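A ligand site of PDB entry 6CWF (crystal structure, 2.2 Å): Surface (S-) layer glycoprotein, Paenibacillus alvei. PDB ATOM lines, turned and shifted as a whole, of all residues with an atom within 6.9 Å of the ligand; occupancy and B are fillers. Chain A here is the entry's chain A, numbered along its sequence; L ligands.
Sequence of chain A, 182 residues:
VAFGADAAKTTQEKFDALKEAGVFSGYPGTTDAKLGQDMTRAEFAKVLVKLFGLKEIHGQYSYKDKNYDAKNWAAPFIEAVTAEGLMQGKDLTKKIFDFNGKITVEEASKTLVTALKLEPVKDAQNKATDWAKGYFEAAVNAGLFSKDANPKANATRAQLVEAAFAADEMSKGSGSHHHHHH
The guanidinium group (NH2) of Arg 41 lies within salt-bridge range of an oxygen (O4) of the ligand (2.6 Å). N of Gln 88 is in hydrogen-bond range of O5 of the ligand (2.7 Å). The backbone carbonyl oxygen of Gly 89 lies within hydrogen-bond range of a nitrogen (N1) of the ligand (3.1 Å). An oxygen (O5) of the ligand is in salt-bridge range of the side-chain amino group of Lys 110, 3.1 Å away. An oxygen (O4) of the ligand sits at hydrogen-bond distance from the backbone NH (N) of Gly 89. O2 of the ligand sits at hydrogen-bond distance from OE1 of Gln 88 (2.9 Å).
The side-chain amino group (NZ) of Lys 90 is in salt-bridge range of the side-chain carboxylate (OE2) of Glu 107 (3.7 Å). OE1 of Glu 107 is in salt-bridge range of NH1 of Arg 41 (3.0 Å). N of Glu 107 sits close to OG1 of Thr 104, 3.2 Å away. NH2 of Arg 41 sits at hydrogen-bond distance from O of Phe 97, 2.9 Å away. N of Lys 90 lies within hydrogen-bond range of O of Ile 96 (2.9 Å). The backbone carbonyl oxygen of Gln 88 lies close to the side-chain hydroxyl of Tyr 63, at 3.5 Å.
O8 of the ligand lies close to O of Lys 90 (3.4 Å). Merely in contact with the ligand: Leu 92, Met 87, Glu 107 and Trp 131. Within 4 Å of the ligand: Arg 41, Met 87, Gln 88, Gly 89, Lys 90, Leu 92, Glu 107, Lys 110 and Trp 131.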
ATOM      1  N   ARG A  41      -4.914  24.701   4.107  1.00  0.00           N
ATOM      2  CA  ARG A  41      -5.275  23.459   4.712  1.00  0.00           C
ATOM      3  C   ARG A  41      -5.368  22.349   3.658  1.00  0.00           C
ATOM      4  O   ARG A  41      -5.081  21.215   3.967  1.00  0.00           O
ATOM      5  CB  ARG A  41      -6.567  23.568   5.500  1.00  0.00           C
ATOM      6  CG  ARG A  41      -6.382  24.466   6.737  1.00  0.00           C
ATOM      7  CD  ARG A  41      -7.740  24.944   7.227  1.00  0.00           C
ATOM      8  NE  ARG A  41      -8.712  23.840   7.369  1.00  0.00           N
ATOM      9  CZ  ARG A  41      -8.671  22.937   8.345  1.00  0.00           C
ATOM     10  NH1 ARG A  41      -7.684  22.946   9.223  1.00  0.00           N
ATOM     11  NH2 ARG A  41      -9.613  22.001   8.444  1.00  0.00           N
ATOM     12  N   PHE A  44      -1.701  21.307   3.155  1.00  0.00           N
ATOM     13  CA  PHE A  44      -1.261  20.546   4.298  1.00  0.00           C
ATOM     14  C   PHE A  44      -1.800  19.135   4.327  1.00  0.00           C
ATOM     15  O   PHE A  44      -1.171  18.204   4.847  1.00  0.00           O
ATOM     16  CB  PHE A  44      -1.647  21.263   5.602  1.00  0.00           C
ATOM     17  CG  PHE A  44      -0.977  20.705   6.820  1.00  0.00           C
ATOM     18  CD1 PHE A  44       0.389  20.724   6.910  1.00  0.00           C
ATOM     19  CD2 PHE A  44      -1.691  20.117   7.822  1.00  0.00           C
ATOM     20  CE1 PHE A  44       1.042  20.181   7.961  1.00  0.00           C
ATOM     21  CE2 PHE A  44      -1.054  19.566   8.887  1.00  0.00           C
ATOM     22  CZ  PHE A  44       0.328  19.607   8.966  1.00  0.00           C
ATOM     23  N   TYR A  63     -17.318  16.783   2.351  1.00  0.00           N
ATOM     24  CA  TYR A  63     -17.502  18.168   2.780  1.00  0.00           C
ATOM     25  C   TYR A  63     -18.273  18.958   1.729  1.00  0.00           C
ATOM     26  O   TYR A  63     -18.375  18.540   0.565  1.00  0.00           O
ATOM     27  CB  TYR A  63     -16.155  18.847   3.070  1.00  0.00           C
ATOM     28  CG  TYR A  63     -15.333  18.154   4.135  1.00  0.00           C
ATOM     29  CD1 TYR A  63     -15.653  18.270   5.488  1.00  0.00           C
ATOM     30  CD2 TYR A  63     -14.189  17.367   3.784  1.00  0.00           C
ATOM     31  CE1 TYR A  63     -14.882  17.646   6.479  1.00  0.00           C
ATOM     32  CE2 TYR A  63     -13.433  16.701   4.763  1.00  0.00           C
ATOM     33  CZ  TYR A  63     -13.757  16.853   6.117  1.00  0.00           C
ATOM     34  OH  TYR A  63     -12.999  16.216   7.099  1.00  0.00           O
ATOM     35  N   GLY A  85      -8.490  10.045  10.042  1.00  0.00           N
ATOM     36  CA  GLY A  85      -8.764  10.624  11.334  1.00  0.00           C
ATOM     37  C   GLY A  85      -7.820  11.748  11.767  1.00  0.00           C
ATOM     38  O   GLY A  85      -7.888  12.201  12.926  1.00  0.00           O
ATOM     39  N   LEU A  86      -6.967  12.226  10.859  1.00  0.00           N
ATOM     40  CA  LEU A  86      -6.071  13.311  11.162  1.00  0.00           C
ATOM     41  C   LEU A  86      -6.756  14.663  11.100  1.00  0.00           C
ATOM     42  O   LEU A  86      -6.374  15.618  11.834  1.00  0.00           O
ATOM     43  CB  LEU A  86      -4.917  13.307  10.210  1.00  0.00           C
ATOM     44  CG  LEU A  86      -4.114  12.010  10.147  1.00  0.00           C
ATOM     45  CD1 LEU A  86      -2.857  12.228   9.319  1.00  0.00           C
ATOM     46  CD2 LEU A  86      -3.760  11.524  11.559  1.00  0.00           C
ATOM     47  N   MET A  87      -7.745  14.801  10.237  1.00  0.00           N
ATOM     48  CA  MET A  87      -8.471  16.046  10.188  1.00  0.00           C
ATOM     49  C   MET A  87      -9.965  15.757  10.012  1.00  0.00           C
ATOM     50  O   MET A  87     -10.337  14.703   9.488  1.00  0.00           O
ATOM     51  CB  MET A  87      -7.951  16.928   9.060  1.00  0.00           C
ATOM     52  CG  MET A  87      -6.436  17.217   9.054  1.00  0.00           C
ATOM     53  SD  MET A  87      -5.886  18.155   7.597  1.00  0.00           S
ATOM     54  CE  MET A  87      -6.363  19.839   8.053  1.00  0.00           C
ATOM     55  N   GLN A  88     -10.791  16.689  10.488  1.00  0.00           N
ATOM     56  CA  GLN A  88     -12.247  16.634  10.426  1.00  0.00           C
ATOM     57  C   GLN A  88     -12.926  17.960  10.002  1.00  0.00           C
ATOM     58  O   GLN A  88     -14.132  17.995   9.842  1.00  0.00           O
ATOM     59  CB  GLN A  88     -12.846  16.087  11.742  1.00  0.00           C
ATOM     60  CG  GLN A  88     -12.034  16.398  12.992  1.00  0.00           C
ATOM     61  CD  GLN A  88     -12.879  16.975  14.122  1.00  0.00           C
ATOM     62  OE1 GLN A  88     -12.620  18.074  14.660  1.00  0.00           O
ATOM     63  NE2 GLN A  88     -13.912  16.208  14.496  1.00  0.00           N
ATOM     64  N   GLY A  89     -12.182  18.992   9.653  1.00  0.00           N
ATOM     65  CA  GLY A  89     -12.842  20.235   9.207  1.00  0.00           C
ATOM     66  C   GLY A  89     -13.290  21.099  10.382  1.00  0.00           C
ATOM     67  O   GLY A  89     -13.122  20.703  11.537  1.00  0.00           O
ATOM     68  N   LYS A  90     -13.879  22.257  10.078  1.00  0.00           N
ATOM     69  CA  LYS A  90     -14.054  23.317  11.099  1.00  0.00           C
ATOM     70  C   LYS A  90     -15.454  23.342  11.676  1.00  0.00           C
ATOM     71  O   LYS A  90     -15.724  24.089  12.603  1.00  0.00           O
ATOM     72  CB  LYS A  90     -13.722  24.713  10.519  1.00  0.00           C
ATOM     73  CG  LYS A  90     -12.467  24.861   9.682  1.00  0.00           C
ATOM     74  CD  LYS A  90     -11.250  25.279  10.487  1.00  0.00           C
ATOM     75  CE  LYS A  90     -10.931  26.766  10.374  1.00  0.00           C
ATOM     76  NZ  LYS A  90     -10.165  27.155   9.184  1.00  0.00           N
ATOM     77  N   ASP A  91     -16.377  22.571  11.099  1.00  0.00           N
ATOM     78  CA  ASP A  91     -17.735  22.504  11.608  1.00  0.00           C
ATOM     79  C   ASP A  91     -18.433  21.230  11.116  1.00  0.00           C
ATOM     80  O   ASP A  91     -18.659  21.079   9.905  1.00  0.00           O
ATOM     81  CB  ASP A  91     -18.452  23.769  11.123  1.00  0.00           C
ATOM     82  CG  ASP A  91     -19.954  23.766  11.394  1.00  0.00           C
ATOM     83  OD1 ASP A  91     -20.539  22.719  11.711  1.00  0.00           O
ATOM     84  OD2 ASP A  91     -20.531  24.842  11.223  1.00  0.00           O
ATOM     85  N   LEU A  92     -18.764  20.312  12.021  1.00  0.00           N
ATOM     86  CA  LEU A  92     -19.358  19.038  11.606  1.00  0.00           C
ATOM     87  C   LEU A  92     -20.773  19.213  11.024  1.00  0.00           C
ATOM     88  O   LEU A  92     -21.125  18.550  10.054  1.00  0.00           O
ATOM     89  CB  LEU A  92     -19.435  18.025  12.746  1.00  0.00           C
ATOM     90  CG  LEU A  92     -18.125  17.496  13.338  1.00  0.00           C
ATOM     91  CD1 LEU A  92     -17.005  17.265  12.332  1.00  0.00           C
ATOM     92  CD2 LEU A  92     -17.714  18.516  14.343  1.00  0.00           C
ATOM     93  N   ILE A  96     -17.964  21.974   6.672  1.00  0.00           N
ATOM     94  CA  ILE A  96     -16.988  22.845   6.007  1.00  0.00           C
ATOM     95  C   ILE A  96     -15.601  22.378   6.430  1.00  0.00           C
ATOM     96  O   ILE A  96     -15.367  22.096   7.620  1.00  0.00           O
ATOM     97  CB  ILE A  96     -17.232  24.332   6.326  1.00  0.00           C
ATOM     98  CG1 ILE A  96     -18.656  24.742   5.856  1.00  0.00           C
ATOM     99  CG2 ILE A  96     -16.231  25.213   5.630  1.00  0.00           C
ATOM    100  CD1 ILE A  96     -18.906  24.680   4.348  1.00  0.00           C
ATOM    101  N   PHE A  97     -14.728  22.180   5.446  1.00  0.00           N
ATOM    102  CA  PHE A  97     -13.340  21.859   5.738  1.00  0.00           C
ATOM    103  C   PHE A  97     -12.442  23.119   5.789  1.00  0.00           C
ATOM    104  O   PHE A  97     -11.450  23.130   6.488  1.00  0.00           O
ATOM    105  CB  PHE A  97     -12.767  20.913   4.664  1.00  0.00           C
ATOM    106  CG  PHE A  97     -11.403  20.342   5.018  1.00  0.00           C
ATOM    107  CD1 PHE A  97     -11.277  19.386   5.987  1.00  0.00           C
ATOM    108  CD2 PHE A  97     -10.278  20.803   4.386  1.00  0.00           C
ATOM    109  CE1 PHE A  97     -10.044  18.836   6.320  1.00  0.00           C
ATOM    110  CE2 PHE A  97      -9.016  20.275   4.714  1.00  0.00           C
ATOM    111  CZ  PHE A  97      -8.907  19.291   5.682  1.00  0.00           C
ATOM    112  N   ILE A 103      -3.533  26.703   7.311  1.00  0.00           N
ATOM    113  CA  ILE A 103      -3.288  25.852   8.490  1.00  0.00           C
ATOM    114  C   ILE A 103      -2.523  26.632   9.597  1.00  0.00           C
ATOM    115  O   ILE A 103      -1.506  27.324   9.319  1.00  0.00           O
ATOM    116  CB  ILE A 103      -2.492  24.577   8.085  1.00  0.00           C
ATOM    117  CG1 ILE A 103      -2.470  23.543   9.196  1.00  0.00           C
ATOM    118  CG2 ILE A 103      -1.068  24.875   7.648  1.00  0.00           C
ATOM    119  CD1 ILE A 103      -3.666  22.632   9.175  1.00  0.00           C
ATOM    120  N   THR A 104      -3.016  26.470  10.829  1.00  0.00           N
ATOM    121  CA  THR A 104      -2.493  27.172  12.005  1.00  0.00           C
ATOM    122  C   THR A 104      -1.631  26.163  12.741  1.00  0.00           C
ATOM    123  O   THR A 104      -1.694  24.926  12.448  1.00  0.00           O
ATOM    124  CB  THR A 104      -3.599  27.632  12.952  1.00  0.00           C
ATOM    125  OG1 THR A 104      -4.381  26.490  13.338  1.00  0.00           O
ATOM    126  CG2 THR A 104      -4.524  28.636  12.275  1.00  0.00           C
ATOM    127  N   GLU A 106      -1.694  25.251  15.871  1.00  0.00           N
ATOM    128  CA  GLU A 106      -2.457  24.332  16.687  1.00  0.00           C
ATOM    129  C   GLU A 106      -3.223  23.267  15.854  1.00  0.00           C
ATOM    130  O   GLU A 106      -3.384  22.161  16.295  1.00  0.00           O
ATOM    131  CB  GLU A 106      -3.392  25.116  17.566  1.00  0.00           C
ATOM    132  CG  GLU A 106      -4.506  25.843  16.815  1.00  0.00           C
ATOM    133  CD  GLU A 106      -5.328  26.745  17.744  1.00  0.00           C
ATOM    134  OE1 GLU A 106      -5.015  26.807  18.956  1.00  0.00           O
ATOM    135  OE2 GLU A 106      -6.295  27.369  17.263  1.00  0.00           O
ATOM    136  N   GLU A 107      -3.716  23.635  14.674  1.00  0.00           N
ATOM    137  CA  GLU A 107      -4.324  22.706  13.746  1.00  0.00           C
ATOM    138  C   GLU A 107      -3.271  21.667  13.320  1.00  0.00           C
ATOM    139  O   GLU A 107      -3.505  20.493  13.421  1.00  0.00           O
ATOM    140  CB  GLU A 107      -4.960  23.414  12.507  1.00  0.00           C
ATOM    141  CG  GLU A 107      -6.283  24.172  12.750  1.00  0.00           C
ATOM    142  CD  GLU A 107      -6.695  25.003  11.550  1.00  0.00           C
ATOM    143  OE1 GLU A 107      -5.984  25.005  10.561  1.00  0.00           O
ATOM    144  OE2 GLU A 107      -7.719  25.692  11.522  1.00  0.00           O
ATOM    145  N   ALA A 108      -2.098  22.114  12.904  1.00  0.00           N
ATOM    146  CA  ALA A 108      -1.013  21.242  12.558  1.00  0.00           C
ATOM    147  C   ALA A 108      -0.630  20.389  13.718  1.00  0.00           C
ATOM    148  O   ALA A 108      -0.431  19.170  13.541  1.00  0.00           O
ATOM    149  CB  ALA A 108       0.195  22.029  12.095  1.00  0.00           C
ATOM    150  N   LYS A 110      -2.563  19.295  16.058  1.00  0.00           N
ATOM    151  CA  LYS A 110      -3.549  18.215  16.184  1.00  0.00           C
ATOM    152  C   LYS A 110      -3.221  17.085  15.224  1.00  0.00           C
ATOM    153  O   LYS A 110      -3.118  15.930  15.638  1.00  0.00           O
ATOM    154  CB  LYS A 110      -4.957  18.695  15.945  1.00  0.00           C
ATOM    155  CG  LYS A 110      -5.968  17.544  15.904  1.00  0.00           C
ATOM    156  CD  LYS A 110      -7.420  17.993  15.979  1.00  0.00           C
ATOM    157  CE  LYS A 110      -8.108  18.006  14.613  1.00  0.00           C
ATOM    158  NZ  LYS A 110      -8.905  16.820  14.238  1.00  0.00           N
ATOM    159  N   THR A 111      -3.024  17.377  13.942  1.00  0.00           N
ATOM    160  CA  THR A 111      -2.825  16.311  12.966  1.00  0.00           C
ATOM    161  C   THR A 111      -1.606  15.453  13.315  1.00  0.00           C
ATOM    162  O   THR A 111      -1.656  14.227  13.155  1.00  0.00           O
ATOM    163  CB  THR A 111      -2.690  16.815  11.551  1.00  0.00           C
ATOM    164  OG1 THR A 111      -1.469  17.558  11.430  1.00  0.00           O
ATOM    165  CG2 THR A 111      -3.848  17.687  11.134  1.00  0.00           C
ATOM    166  N   TRP A 131     -10.175  23.820  22.375  1.00  0.00           N
ATOM    167  CA  TRP A 131     -10.110  22.470  21.762  1.00  0.00           C
ATOM    168  C   TRP A 131      -8.669  21.996  21.499  1.00  0.00           C
ATOM    169  O   TRP A 131      -8.381  20.819  21.531  1.00  0.00           O
ATOM    170  CB  TRP A 131     -10.924  22.369  20.432  1.00  0.00           C
ATOM    171  CG  TRP A 131     -10.412  23.253  19.289  1.00  0.00           C
ATOM    172  CD1 TRP A 131     -10.849  24.515  18.973  1.00  0.00           C
ATOM    173  CD2 TRP A 131      -9.368  22.953  18.339  1.00  0.00           C
ATOM    174  NE1 TRP A 131     -10.136  25.013  17.892  1.00  0.00           N
ATOM    175  CE2 TRP A 131      -9.217  24.075  17.498  1.00  0.00           C
ATOM    176  CE3 TRP A 131      -8.534  21.836  18.141  1.00  0.00           C
ATOM    177  CZ2 TRP A 131      -8.286  24.112  16.447  1.00  0.00           C
ATOM    178  CZ3 TRP A 131      -7.606  21.878  17.111  1.00  0.00           C
ATOM    179  CH2 TRP A 131      -7.496  23.008  16.273  1.00  0.00           C
ATOM    180  N   TYR A 135      -3.565  19.170  22.387  1.00  0.00           N
ATOM    181  CA  TYR A 135      -2.766  18.848  21.227  1.00  0.00           C
ATOM    182  C   TYR A 135      -1.520  19.728  21.191  1.00  0.00           C
ATOM    183  O   TYR A 135      -0.422  19.204  21.139  1.00  0.00           O
ATOM    184  CB  TYR A 135      -3.595  19.031  19.966  1.00  0.00           C
ATOM    185  CG  TYR A 135      -4.739  18.038  19.794  1.00  0.00           C
ATOM    186  CD1 TYR A 135      -4.517  16.655  19.837  1.00  0.00           C
ATOM    187  CD2 TYR A 135      -6.044  18.488  19.537  1.00  0.00           C
ATOM    188  CE1 TYR A 135      -5.561  15.752  19.659  1.00  0.00           C
ATOM    189  CE2 TYR A 135      -7.092  17.598  19.369  1.00  0.00           C
ATOM    190  CZ  TYR A 135      -6.845  16.240  19.428  1.00  0.00           C
ATOM    191  OH  TYR A 135      -7.904  15.370  19.223  1.00  0.00           O
HETATM  192  C1  LIG L   1     -15.144  20.222  14.407  1.00  0.00           C
HETATM  193  C2  LIG L   1     -14.063  20.896  15.248  1.00  0.00           C
HETATM  194  O1  LIG L   1     -14.127  20.941  16.477  1.00  0.00           O
HETATM  195  N1  LIG L   1     -13.046  21.370  14.550  1.00  0.00           N
HETATM  196  C3  LIG L   1     -11.919  22.053  15.257  1.00  0.00           C
HETATM  197  C4  LIG L   1     -10.551  21.300  15.083  1.00  0.00           C
HETATM  198  O2  LIG L   1     -10.527  19.914  15.590  1.00  0.00           O
HETATM  199  C5  LIG L   1     -10.191  21.265  13.636  1.00  0.00           C
HETATM  200  O3  LIG L   1      -8.924  20.695  13.508  1.00  0.00           O
HETATM  201  C6  LIG L   1      -8.374  20.620  12.212  1.00  0.00           C
HETATM  202  C7  LIG L   1      -6.925  20.074  12.341  1.00  0.00           C
HETATM  203  C8  LIG L   1      -9.167  19.680  11.299  1.00  0.00           C
HETATM  204  O4  LIG L   1      -9.386  20.067  10.117  1.00  0.00           O
HETATM  205  O5  LIG L   1      -9.605  18.681  11.868  1.00  0.00           O
HETATM  206  O6  LIG L   1      -8.434  21.905  11.551  1.00  0.00           O
HETATM  207  C9  LIG L   1      -9.559  22.748  11.737  1.00  0.00           C
HETATM  208  C10 LIG L   1     -10.111  22.664  13.162  1.00  0.00           C
HETATM  209  O7  LIG L   1     -11.382  23.311  13.250  1.00  0.00           O
HETATM  210  C11 LIG L   1     -11.814  23.441  14.637  1.00  0.00           C
HETATM  211  O8  LIG L   1     -13.099  24.135  14.700  1.00  0.00           O
HETATM  212  C12 LIG L   1     -13.001  25.501  14.199  1.00  0.00           C
